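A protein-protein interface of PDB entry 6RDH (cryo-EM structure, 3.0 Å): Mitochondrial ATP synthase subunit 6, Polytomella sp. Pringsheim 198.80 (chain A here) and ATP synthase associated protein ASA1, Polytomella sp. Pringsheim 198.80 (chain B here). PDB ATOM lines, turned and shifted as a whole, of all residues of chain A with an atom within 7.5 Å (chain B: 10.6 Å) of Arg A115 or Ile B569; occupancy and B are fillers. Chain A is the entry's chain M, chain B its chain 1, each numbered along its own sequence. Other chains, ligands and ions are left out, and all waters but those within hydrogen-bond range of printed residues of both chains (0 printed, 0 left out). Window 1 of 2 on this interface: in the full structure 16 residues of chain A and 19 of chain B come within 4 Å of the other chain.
The guanidinium group (NH1) of Arg A118 lies within salt-bridge range of the side-chain carboxylate (OD2) of Asp B573 (2.9 Å). The guanidinium group (NH2) of Arg A118 sits at hydrogen-bond distance from the side-chain hydroxyl (OG1) of Thr B570 (2.8 Å). The side-chain carboxylate (OD2) of Asp B566 is in salt-bridge range of the guanidinium group (NH2) of Arg A118.
Of the 17 printed residues of chain A, 5 touch a printed residue of chain B. Along chain A the printed residues that touch a printed residue of chain B span positions 114 to 123. Of the 19 printed residues of chain B, 6 touch a printed residue of chain A. Hydrophobic or aromatic side chains of chain B within 4 Å of the printed part of chain A: Ile B569 and Met B574. Among the printed residues, 9 pairs touch across the chains.
No residue of chain B comes within 4 Å of Gly A112. No residue of chain B comes within 4 Å of Ser A119. Of the printed residues of chain B, Pro A122 touches Asp B573 (3.6 Å). Printed residues of chain A within 4 Å of Ile B569: Arg A115. Of the printed residues of chain A, Thr B570 touches Arg A118.
Among the printed residues, merely in contact across the chains: Pro A122 with Asp B573 (3.6 Å), Tyr A114 with Glu B565 (3.6 Å), Ala A123 with Asp B573 (3.7 Å), Arg A115 with Ile B569 (3.8 Å), Tyr A114 with Asp B566 (3.9 Å) and Ala A123 with Met B574 (3.97 Å).
The backbone carbonyl oxygen of Glu B559 is in hydrogen-bond range of the backbone NH of Glu B565 (3.2 Å). OG1 of Thr B570 sits at hydrogen-bond distance from O of Asp B566, 2.9 Å away.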
ATOM      1  N   ASN A 108      12.426  -0.940   3.587  1.00  0.00           N
ATOM      2  CA  ASN A 108      12.438  -2.242   2.927  1.00  0.00           C
ATOM      3  C   ASN A 108      13.850  -2.794   2.807  1.00  0.00           C
ATOM      4  O   ASN A 108      14.087  -3.984   3.047  1.00  0.00           O
ATOM      5  CB  ASN A 108      11.810  -2.131   1.548  1.00  0.00           C
ATOM      6  CG  ASN A 108      10.378  -1.739   1.596  1.00  0.00           C
ATOM      7  OD1 ASN A 108       9.867  -1.108   0.680  1.00  0.00           O
ATOM      8  ND2 ASN A 108       9.711  -2.090   2.675  1.00  0.00           N
ATOM      9  N   PHE A 109      14.805  -1.933   2.457  1.00  0.00           N
ATOM     10  CA  PHE A 109      16.187  -2.367   2.313  1.00  0.00           C
ATOM     11  C   PHE A 109      16.783  -2.780   3.647  1.00  0.00           C
ATOM     12  O   PHE A 109      17.406  -3.836   3.744  1.00  0.00           O
ATOM     13  CB  PHE A 109      17.014  -1.258   1.684  1.00  0.00           C
ATOM     14  CG  PHE A 109      18.449  -1.614   1.494  1.00  0.00           C
ATOM     15  CD1 PHE A 109      18.810  -2.639   0.650  1.00  0.00           C
ATOM     16  CD2 PHE A 109      19.440  -0.911   2.143  1.00  0.00           C
ATOM     17  CE1 PHE A 109      20.123  -2.964   0.470  1.00  0.00           C
ATOM     18  CE2 PHE A 109      20.755  -1.238   1.964  1.00  0.00           C
ATOM     19  CZ  PHE A 109      21.095  -2.262   1.129  1.00  0.00           C
ATOM     20  N   LEU A 110      16.583  -1.981   4.693  1.00  0.00           N
ATOM     21  CA  LEU A 110      17.116  -2.341   5.998  1.00  0.00           C
ATOM     22  C   LEU A 110      16.392  -3.529   6.605  1.00  0.00           C
ATOM     23  O   LEU A 110      16.994  -4.268   7.383  1.00  0.00           O
ATOM     24  CB  LEU A 110      17.047  -1.156   6.949  1.00  0.00           C
ATOM     25  CG  LEU A 110      18.332  -0.382   7.201  1.00  0.00           C
ATOM     26  CD1 LEU A 110      19.280  -1.275   7.953  1.00  0.00           C
ATOM     27  CD2 LEU A 110      18.961   0.119   5.933  1.00  0.00           C
ATOM     28  N   THR A 111      15.123  -3.747   6.256  1.00  0.00           N
ATOM     29  CA  THR A 111      14.430  -4.957   6.682  1.00  0.00           C
ATOM     30  C   THR A 111      15.059  -6.188   6.061  1.00  0.00           C
ATOM     31  O   THR A 111      15.325  -7.177   6.751  1.00  0.00           O
ATOM     32  CB  THR A 111      12.963  -4.878   6.296  1.00  0.00           C
ATOM     33  OG1 THR A 111      12.410  -3.654   6.775  1.00  0.00           O
ATOM     34  CG2 THR A 111      12.206  -6.023   6.892  1.00  0.00           C
ATOM     35  N   GLY A 112      15.323  -6.132   4.756  1.00  0.00           N
ATOM     36  CA  GLY A 112      15.971  -7.248   4.091  1.00  0.00           C
ATOM     37  C   GLY A 112      17.381  -7.489   4.583  1.00  0.00           C
ATOM     38  O   GLY A 112      17.794  -8.635   4.759  1.00  0.00           O
ATOM     39  N   VAL A 113      18.114  -6.413   4.872  1.00  0.00           N
ATOM     40  CA  VAL A 113      19.488  -6.536   5.346  1.00  0.00           C
ATOM     41  C   VAL A 113      19.524  -7.130   6.747  1.00  0.00           C
ATOM     42  O   VAL A 113      20.280  -8.071   7.010  1.00  0.00           O
ATOM     43  CB  VAL A 113      20.191  -5.171   5.284  1.00  0.00           C
ATOM     44  CG1 VAL A 113      21.449  -5.177   6.080  1.00  0.00           C
ATOM     45  CG2 VAL A 113      20.520  -4.832   3.872  1.00  0.00           C
ATOM     46  N   TYR A 114      18.684  -6.620   7.654  1.00  0.00           N
ATOM     47  CA  TYR A 114      18.646  -7.138   9.016  1.00  0.00           C
ATOM     48  C   TYR A 114      18.189  -8.583   9.059  1.00  0.00           C
ATOM     49  O   TYR A 114      18.737  -9.382   9.820  1.00  0.00           O
ATOM     50  CB  TYR A 114      17.724  -6.291   9.886  1.00  0.00           C
ATOM     51  CG  TYR A 114      17.558  -6.860  11.271  1.00  0.00           C
ATOM     52  CD1 TYR A 114      18.581  -6.778  12.186  1.00  0.00           C
ATOM     53  CD2 TYR A 114      16.386  -7.494  11.655  1.00  0.00           C
ATOM     54  CE1 TYR A 114      18.451  -7.298  13.435  1.00  0.00           C
ATOM     55  CE2 TYR A 114      16.257  -8.028  12.907  1.00  0.00           C
ATOM     56  CZ  TYR A 114      17.294  -7.915  13.792  1.00  0.00           C
ATOM     57  OH  TYR A 114      17.183  -8.429  15.053  1.00  0.00           O
ATOM     58  N   ARG A 115      17.195  -8.946   8.251  1.00  0.00           N
ATOM     59  CA  ARG A 115      16.747 -10.329   8.253  1.00  0.00           C
ATOM     60  C   ARG A 115      17.770 -11.252   7.615  1.00  0.00           C
ATOM     61  O   ARG A 115      17.880 -12.412   8.026  1.00  0.00           O
ATOM     62  CB  ARG A 115      15.409 -10.435   7.547  1.00  0.00           C
ATOM     63  CG  ARG A 115      14.271  -9.908   8.371  1.00  0.00           C
ATOM     64  CD  ARG A 115      13.013  -9.831   7.568  1.00  0.00           C
ATOM     65  NE  ARG A 115      12.727 -11.099   6.929  1.00  0.00           N
ATOM     66  CZ  ARG A 115      12.064 -12.084   7.511  1.00  0.00           C
ATOM     67  NH1 ARG A 115      11.844 -13.210   6.857  1.00  0.00           N
ATOM     68  NH2 ARG A 115      11.619 -11.944   8.744  1.00  0.00           N
ATOM     69  N   PHE A 116      18.569 -10.746   6.670  1.00  0.00           N
ATOM     70  CA  PHE A 116      19.670 -11.535   6.133  1.00  0.00           C
ATOM     71  C   PHE A 116      20.718 -11.821   7.191  1.00  0.00           C
ATOM     72  O   PHE A 116      21.158 -12.961   7.345  1.00  0.00           O
ATOM     73  CB  PHE A 116      20.321 -10.823   4.958  1.00  0.00           C
ATOM     74  CG  PHE A 116      21.400 -11.623   4.297  1.00  0.00           C
ATOM     75  CD1 PHE A 116      21.082 -12.622   3.407  1.00  0.00           C
ATOM     76  CD2 PHE A 116      22.729 -11.374   4.558  1.00  0.00           C
ATOM     77  CE1 PHE A 116      22.067 -13.351   2.800  1.00  0.00           C
ATOM     78  CE2 PHE A 116      23.710 -12.105   3.959  1.00  0.00           C
ATOM     79  CZ  PHE A 116      23.382 -13.087   3.079  1.00  0.00           C
ATOM     80  N   TRP A 117      21.145 -10.798   7.922  1.00  0.00           N
ATOM     81  CA  TRP A 117      22.182 -11.029   8.918  1.00  0.00           C
ATOM     82  C   TRP A 117      21.667 -11.734  10.151  1.00  0.00           C
ATOM     83  O   TRP A 117      22.460 -12.315  10.888  1.00  0.00           O
ATOM     84  CB  TRP A 117      22.853  -9.723   9.323  1.00  0.00           C
ATOM     85  CG  TRP A 117      23.531  -9.055   8.202  1.00  0.00           C
ATOM     86  CD1 TRP A 117      23.232  -7.850   7.686  1.00  0.00           C
ATOM     87  CD2 TRP A 117      24.631  -9.553   7.440  1.00  0.00           C
ATOM     88  NE1 TRP A 117      24.058  -7.559   6.647  1.00  0.00           N
ATOM     89  CE2 TRP A 117      24.930  -8.593   6.475  1.00  0.00           C
ATOM     90  CE3 TRP A 117      25.390 -10.718   7.480  1.00  0.00           C
ATOM     91  CZ2 TRP A 117      25.945  -8.757   5.564  1.00  0.00           C
ATOM     92  CZ3 TRP A 117      26.381 -10.881   6.578  1.00  0.00           C
ATOM     93  CH2 TRP A 117      26.649  -9.912   5.625  1.00  0.00           C
ATOM     94  N   ARG A 118      20.366 -11.701  10.392  1.00  0.00           N
ATOM     95  CA  ARG A 118      19.801 -12.473  11.481  1.00  0.00           C
ATOM     96  C   ARG A 118      19.644 -13.934  11.089  1.00  0.00           C
ATOM     97  O   ARG A 118      19.784 -14.817  11.935  1.00  0.00           O
ATOM     98  CB  ARG A 118      18.482 -11.830  11.905  1.00  0.00           C
ATOM     99  CG  ARG A 118      17.583 -12.633  12.796  1.00  0.00           C
ATOM    100  CD  ARG A 118      18.214 -12.966  14.118  1.00  0.00           C
ATOM    101  NE  ARG A 118      17.338 -13.794  14.934  1.00  0.00           N
ATOM    102  CZ  ARG A 118      17.194 -15.103  14.800  1.00  0.00           C
ATOM    103  NH1 ARG A 118      17.862 -15.765  13.879  1.00  0.00           N
ATOM    104  NH2 ARG A 118      16.373 -15.757  15.596  1.00  0.00           N
ATOM    105  N   SER A 119      19.440 -14.223   9.808  1.00  0.00           N
ATOM    106  CA  SER A 119      19.360 -15.610   9.381  1.00  0.00           C
ATOM    107  C   SER A 119      20.703 -16.327   9.340  1.00  0.00           C
ATOM    108  O   SER A 119      20.729 -17.507   8.993  1.00  0.00           O
ATOM    109  CB  SER A 119      18.722 -15.680   8.005  1.00  0.00           C
ATOM    110  OG  SER A 119      19.681 -15.433   7.001  1.00  0.00           O
ATOM    111  N   GLN A 120      21.811 -15.658   9.652  1.00  0.00           N
ATOM    112  CA  GLN A 120      23.110 -16.319   9.595  1.00  0.00           C
ATOM    113  C   GLN A 120      23.326 -17.214  10.800  1.00  0.00           C
ATOM    114  O   GLN A 120      23.923 -18.286  10.684  1.00  0.00           O
ATOM    115  CB  GLN A 120      24.227 -15.287   9.506  1.00  0.00           C
ATOM    116  CG  GLN A 120      24.214 -14.492   8.246  1.00  0.00           C
ATOM    117  CD  GLN A 120      24.273 -15.362   7.037  1.00  0.00           C
ATOM    118  OE1 GLN A 120      23.429 -15.279   6.157  1.00  0.00           O
ATOM    119  NE2 GLN A 120      25.276 -16.211   6.981  1.00  0.00           N
ATOM    120  N   PRO A 122      20.874 -18.859  13.024  1.00  0.00           N
ATOM    121  CA  PRO A 122      19.485 -19.142  13.359  1.00  0.00           C
ATOM    122  C   PRO A 122      19.380 -19.830  14.707  1.00  0.00           C
ATOM    123  O   PRO A 122      20.352 -20.358  15.245  1.00  0.00           O
ATOM    124  CB  PRO A 122      19.045 -20.070  12.232  1.00  0.00           C
ATOM    125  CG  PRO A 122      20.244 -20.796  11.903  1.00  0.00           C
ATOM    126  CD  PRO A 122      21.403 -19.870  12.100  1.00  0.00           C
ATOM    127  N   ALA A 123      18.173 -19.798  15.254  1.00  0.00           N
ATOM    128  CA  ALA A 123      17.917 -20.445  16.524  1.00  0.00           C
ATOM    129  C   ALA A 123      17.874 -21.957  16.344  1.00  0.00           C
ATOM    130  O   ALA A 123      17.822 -22.480  15.229  1.00  0.00           O
ATOM    131  CB  ALA A 123      16.616 -19.942  17.130  1.00  0.00           C
ATOM    132  N   GLY A 149      22.713 -10.519  14.821  1.00  0.00           N
ATOM    133  CA  GLY A 149      21.981  -9.894  13.735  1.00  0.00           C
ATOM    134  C   GLY A 149      22.153  -8.393  13.733  1.00  0.00           C
ATOM    135  O   GLY A 149      22.520  -7.807  12.717  1.00  0.00           O
ATOM    136  N   THR A 153      24.552  -6.305  11.062  1.00  0.00           N
ATOM    137  CA  THR A 153      24.079  -5.250  10.177  1.00  0.00           C
ATOM    138  C   THR A 153      24.633  -3.889  10.552  1.00  0.00           C
ATOM    139  O   THR A 153      24.754  -3.041   9.669  1.00  0.00           O
ATOM    140  CB  THR A 153      22.557  -5.200  10.096  1.00  0.00           C
ATOM    141  OG1 THR A 153      22.177  -4.103   9.269  1.00  0.00           O
ATOM    142  CG2 THR A 153      21.957  -4.990  11.386  1.00  0.00           C
ATOM    143  N   GLU B 559       8.171  -5.835  22.233  1.00  0.00           N
ATOM    144  CA  GLU B 559       9.097  -6.800  21.644  1.00  0.00           C
ATOM    145  C   GLU B 559      10.414  -6.150  21.253  1.00  0.00           C
ATOM    146  O   GLU B 559      11.465  -6.788  21.317  1.00  0.00           O
ATOM    147  CB  GLU B 559       8.486  -7.451  20.421  1.00  0.00           C
ATOM    148  CG  GLU B 559       7.281  -8.237  20.712  1.00  0.00           C
ATOM    149  CD  GLU B 559       6.955  -9.206  19.625  1.00  0.00           C
ATOM    150  OE1 GLU B 559       7.794  -9.383  18.731  1.00  0.00           O
ATOM    151  OE2 GLU B 559       5.865  -9.795  19.660  1.00  0.00           O
ATOM    152  N   ALA B 563      14.262  -6.964  23.615  1.00  0.00           N
ATOM    153  CA  ALA B 563      15.253  -7.699  22.834  1.00  0.00           C
ATOM    154  C   ALA B 563      14.666  -8.855  22.047  1.00  0.00           C
ATOM    155  O   ALA B 563      15.385  -9.786  21.689  1.00  0.00           O
ATOM    156  CB  ALA B 563      16.391  -8.202  23.720  1.00  0.00           C
ATOM    157  N   LEU B 564      13.378  -8.819  21.762  1.00  0.00           N
ATOM    158  CA  LEU B 564      12.703  -9.879  21.036  1.00  0.00           C
ATOM    159  C   LEU B 564      12.225  -9.371  19.692  1.00  0.00           C
ATOM    160  O   LEU B 564      11.172  -9.754  19.203  1.00  0.00           O
ATOM    161  CB  LEU B 564      11.540 -10.433  21.842  1.00  0.00           C
ATOM    162  CG  LEU B 564      11.897 -11.171  23.121  1.00  0.00           C
ATOM    163  CD1 LEU B 564      10.650 -11.360  23.934  1.00  0.00           C
ATOM    164  CD2 LEU B 564      12.512 -12.497  22.779  1.00  0.00           C
ATOM    165  N   GLU B 565      13.017  -8.500  19.078  1.00  0.00           N
ATOM    166  CA  GLU B 565      12.672  -7.918  17.793  1.00  0.00           C
ATOM    167  C   GLU B 565      12.731  -8.927  16.667  1.00  0.00           C
ATOM    168  O   GLU B 565      12.164  -8.687  15.602  1.00  0.00           O
ATOM    169  CB  GLU B 565      13.624  -6.771  17.531  1.00  0.00           C
ATOM    170  CG  GLU B 565      15.032  -7.209  17.725  1.00  0.00           C
ATOM    171  CD  GLU B 565      15.876  -6.158  18.362  1.00  0.00           C
ATOM    172  OE1 GLU B 565      15.379  -5.030  18.540  1.00  0.00           O
ATOM    173  OE2 GLU B 565      17.025  -6.473  18.732  1.00  0.00           O
ATOM    174  N   ASP B 566      13.407 -10.043  16.876  1.00  0.00           N
ATOM    175  CA  ASP B 566      13.448 -11.134  15.923  1.00  0.00           C
ATOM    176  C   ASP B 566      12.649 -12.329  16.415  1.00  0.00           C
ATOM    177  O   ASP B 566      13.022 -13.469  16.151  1.00  0.00           O
ATOM    178  CB  ASP B 566      14.891 -11.541  15.663  1.00  0.00           C
ATOM    179  CG  ASP B 566      15.629 -11.910  16.932  1.00  0.00           C
ATOM    180  OD1 ASP B 566      15.495 -11.201  17.942  1.00  0.00           O
ATOM    181  OD2 ASP B 566      16.350 -12.921  16.922  1.00  0.00           O
ATOM    182  N   PHE B 567      11.553 -12.086  17.136  1.00  0.00           N
ATOM    183  CA  PHE B 567      10.868 -13.197  17.780  1.00  0.00           C
ATOM    184  C   PHE B 567      10.089 -14.031  16.783  1.00  0.00           C
ATOM    185  O   PHE B 567      10.015 -15.251  16.932  1.00  0.00           O
ATOM    186  CB  PHE B 567       9.941 -12.722  18.887  1.00  0.00           C
ATOM    187  CG  PHE B 567       9.381 -13.841  19.703  1.00  0.00           C
ATOM    188  CD1 PHE B 567      10.226 -14.723  20.344  1.00  0.00           C
ATOM    189  CD2 PHE B 567       8.020 -14.028  19.810  1.00  0.00           C
ATOM    190  CE1 PHE B 567       9.726 -15.762  21.081  1.00  0.00           C
ATOM    191  CE2 PHE B 567       7.516 -15.068  20.542  1.00  0.00           C
ATOM    192  CZ  PHE B 567       8.368 -15.934  21.179  1.00  0.00           C
ATOM    193  N   ASP B 568       9.510 -13.416  15.755  1.00  0.00           N
ATOM    194  CA  ASP B 568       8.898 -14.246  14.727  1.00  0.00           C
ATOM    195  C   ASP B 568       9.950 -14.945  13.881  1.00  0.00           C
ATOM    196  O   ASP B 568       9.720 -16.067  13.418  1.00  0.00           O
ATOM    197  CB  ASP B 568       7.958 -13.432  13.851  1.00  0.00           C
ATOM    198  CG  ASP B 568       8.625 -12.261  13.208  1.00  0.00           C
ATOM    199  OD1 ASP B 568       9.340 -11.524  13.906  1.00  0.00           O
ATOM    200  OD2 ASP B 568       8.418 -12.064  11.998  1.00  0.00           O
ATOM    201  N   ILE B 569      11.117 -14.320  13.704  1.00  0.00           N
ATOM    202  CA  ILE B 569      12.223 -14.982  13.027  1.00  0.00           C
ATOM    203  C   ILE B 569      12.739 -16.132  13.864  1.00  0.00           C
ATOM    204  O   ILE B 569      13.120 -17.171  13.324  1.00  0.00           O
ATOM    205  CB  ILE B 569      13.345 -13.985  12.703  1.00  0.00           C
ATOM    206  CG1 ILE B 569      12.763 -12.658  12.249  1.00  0.00           C
ATOM    207  CG2 ILE B 569      14.210 -14.522  11.608  1.00  0.00           C
ATOM    208  CD1 ILE B 569      13.795 -11.596  12.032  1.00  0.00           C
ATOM    209  N   THR B 570      12.745 -15.978  15.188  1.00  0.00           N
ATOM    210  CA  THR B 570      13.113 -17.076  16.072  1.00  0.00           C
ATOM    211  C   THR B 570      12.091 -18.197  15.999  1.00  0.00           C
ATOM    212  O   THR B 570      12.460 -19.370  15.934  1.00  0.00           O
ATOM    213  CB  THR B 570      13.256 -16.559  17.500  1.00  0.00           C
ATOM    214  OG1 THR B 570      14.360 -15.654  17.562  1.00  0.00           O
ATOM    215  CG2 THR B 570      13.497 -17.673  18.470  1.00  0.00           C
ATOM    216  N   LEU B 571      10.809 -17.850  15.924  1.00  0.00           N
ATOM    217  CA  LEU B 571       9.756 -18.856  15.944  1.00  0.00           C
ATOM    218  C   LEU B 571       9.713 -19.662  14.658  1.00  0.00           C
ATOM    219  O   LEU B 571       9.468 -20.869  14.699  1.00  0.00           O
ATOM    220  CB  LEU B 571       8.407 -18.202  16.198  1.00  0.00           C
ATOM    221  CG  LEU B 571       8.127 -17.851  17.647  1.00  0.00           C
ATOM    222  CD1 LEU B 571       6.760 -17.275  17.743  1.00  0.00           C
ATOM    223  CD2 LEU B 571       8.249 -19.072  18.505  1.00  0.00           C
ATOM    224  N   ASP B 572       9.938 -19.039  13.508  1.00  0.00           N
ATOM    225  CA  ASP B 572      10.010 -19.867  12.311  1.00  0.00           C
ATOM    226  C   ASP B 572      11.426 -20.331  11.995  1.00  0.00           C
ATOM    227  O   ASP B 572      11.620 -21.042  11.009  1.00  0.00           O
ATOM    228  CB  ASP B 572       9.377 -19.170  11.097  1.00  0.00           C
ATOM    229  CG  ASP B 572       9.871 -17.762  10.872  1.00  0.00           C
ATOM    230  OD1 ASP B 572      11.018 -17.442  11.219  1.00  0.00           O
ATOM    231  OD2 ASP B 572       9.094 -16.951  10.331  1.00  0.00           O
ATOM    232  N   ASP B 573      12.417 -19.945  12.798  1.00  0.00           N
ATOM    233  CA  ASP B 573      13.705 -20.625  12.736  1.00  0.00           C
ATOM    234  C   ASP B 573      13.636 -21.978  13.415  1.00  0.00           C
ATOM    235  O   ASP B 573      14.310 -22.921  12.991  1.00  0.00           O
ATOM    236  CB  ASP B 573      14.798 -19.778  13.391  1.00  0.00           C
ATOM    237  CG  ASP B 573      15.519 -18.889  12.406  1.00  0.00           C
ATOM    238  OD1 ASP B 573      15.433 -19.151  11.192  1.00  0.00           O
ATOM    239  OD2 ASP B 573      16.174 -17.922  12.842  1.00  0.00           O
ATOM    240  N   MET B 574      12.832 -22.094  14.468  1.00  0.00           N
ATOM    241  CA  MET B 574      12.665 -23.345  15.184  1.00  0.00           C
ATOM    242  C   MET B 574      11.392 -24.069  14.782  1.00  0.00           C
ATOM    243  O   MET B 574      10.894 -24.905  15.540  1.00  0.00           O
ATOM    244  CB  MET B 574      12.707 -23.106  16.692  1.00  0.00           C
ATOM    245  CG  MET B 574      11.635 -22.229  17.243  1.00  0.00           C
ATOM    246  SD  MET B 574      11.835 -22.012  19.006  1.00  0.00           S
ATOM    247  CE  MET B 574      13.551 -21.555  19.079  1.00  0.00           C
ATOM    248  N   GLY B 575      10.856 -23.764  13.604  1.00  0.00           N
ATOM    249  CA  GLY B 575       9.769 -24.524  13.019  1.00  0.00           C
ATOM    250  C   GLY B 575       8.434 -24.419  13.714  1.00  0.00           C
ATOM    251  O   GLY B 575       7.533 -25.199  13.400  1.00  0.00           O
ATOM    252  N   ALA B 576       8.269 -23.483  14.639  1.00  0.00           N
ATOM    253  CA  ALA B 576       7.041 -23.382  15.413  1.00  0.00           C
ATOM    254  C   ALA B 576       5.986 -22.671  14.588  1.00  0.00           C
ATOM    255  O   ALA B 576       6.065 -21.459  14.385  1.00  0.00           O
ATOM    256  CB  ALA B 576       7.301 -22.636  16.713  1.00  0.00           C
ATOM    257  N   GLU B 577       4.994 -23.412  14.108  1.00  0.00           N
ATOM    258  CA  GLU B 577       3.900 -22.790  13.379  1.00  0.00           C
ATOM    259  C   GLU B 577       2.741 -22.426  14.290  1.00  0.00           C
ATOM    260  O   GLU B 577       2.146 -21.356  14.133  1.00  0.00           O
ATOM    261  CB  GLU B 577       3.414 -23.712  12.267  1.00  0.00           C
ATOM    262  CG  GLU B 577       4.407 -23.874  11.141  1.00  0.00           C
ATOM    263  CD  GLU B 577       4.354 -25.251  10.522  1.00  0.00           C
ATOM    264  OE1 GLU B 577       5.338 -25.648   9.861  1.00  0.00           O
ATOM    265  OE2 GLU B 577       3.326 -25.937  10.696  1.00  0.00           O
ATOM    266  N   ALA B 579       2.998 -21.805  17.520  1.00  0.00           N
ATOM    267  CA  ALA B 579       3.427 -20.706  18.370  1.00  0.00           C
ATOM    268  C   ALA B 579       3.505 -19.408  17.590  1.00  0.00           C
ATOM    269  O   ALA B 579       3.301 -18.337  18.160  1.00  0.00           O
ATOM    270  CB  ALA B 579       4.771 -21.021  19.007  1.00  0.00           C
ATOM    271  N   LYS B 580       3.761 -19.483  16.287  1.00  0.00           N
ATOM    272  CA  LYS B 580       3.725 -18.291  15.449  1.00  0.00           C
ATOM    273  C   LYS B 580       2.304 -17.773  15.289  1.00  0.00           C
ATOM    274  O   LYS B 580       2.066 -16.562  15.384  1.00  0.00           O
ATOM    275  CB  LYS B 580       4.338 -18.604  14.093  1.00  0.00           C
ATOM    276  CG  LYS B 580       4.287 -17.480  13.110  1.00  0.00           C
ATOM    277  CD  LYS B 580       5.450 -16.557  13.285  1.00  0.00           C
ATOM    278  CE  LYS B 580       5.677 -15.775  12.026  1.00  0.00           C
ATOM    279  NZ  LYS B 580       5.914 -16.697  10.897  1.00  0.00           N
ATOM    280  N   TRP B 583       1.404 -16.208  18.498  1.00  0.00           N
ATOM    281  CA  TRP B 583       2.037 -14.902  18.642  1.00  0.00           C
ATOM    282  C   TRP B 583       1.261 -13.837  17.884  1.00  0.00           C
ATOM    283  O   TRP B 583       0.980 -12.755  18.418  1.00  0.00           O
ATOM    284  CB  TRP B 583       3.482 -14.991  18.154  1.00  0.00           C
ATOM    285  CG  TRP B 583       4.154 -13.694  17.873  1.00  0.00           C
ATOM    286  CD1 TRP B 583       4.768 -12.878  18.765  1.00  0.00           C
ATOM    287  CD2 TRP B 583       4.305 -13.079  16.600  1.00  0.00           C
ATOM    288  NE1 TRP B 583       5.276 -11.783  18.130  1.00  0.00           N
ATOM    289  CE2 TRP B 583       5.004 -11.887  16.794  1.00  0.00           C
ATOM    290  CE3 TRP B 583       3.907 -13.420  15.312  1.00  0.00           C
ATOM    291  CZ2 TRP B 583       5.306 -11.038  15.756  1.00  0.00           C
ATOM    292  CZ3 TRP B 583       4.209 -12.582  14.294  1.00  0.00           C
ATOM    293  CH2 TRP B 583       4.906 -11.407  14.513  1.00  0.00           C
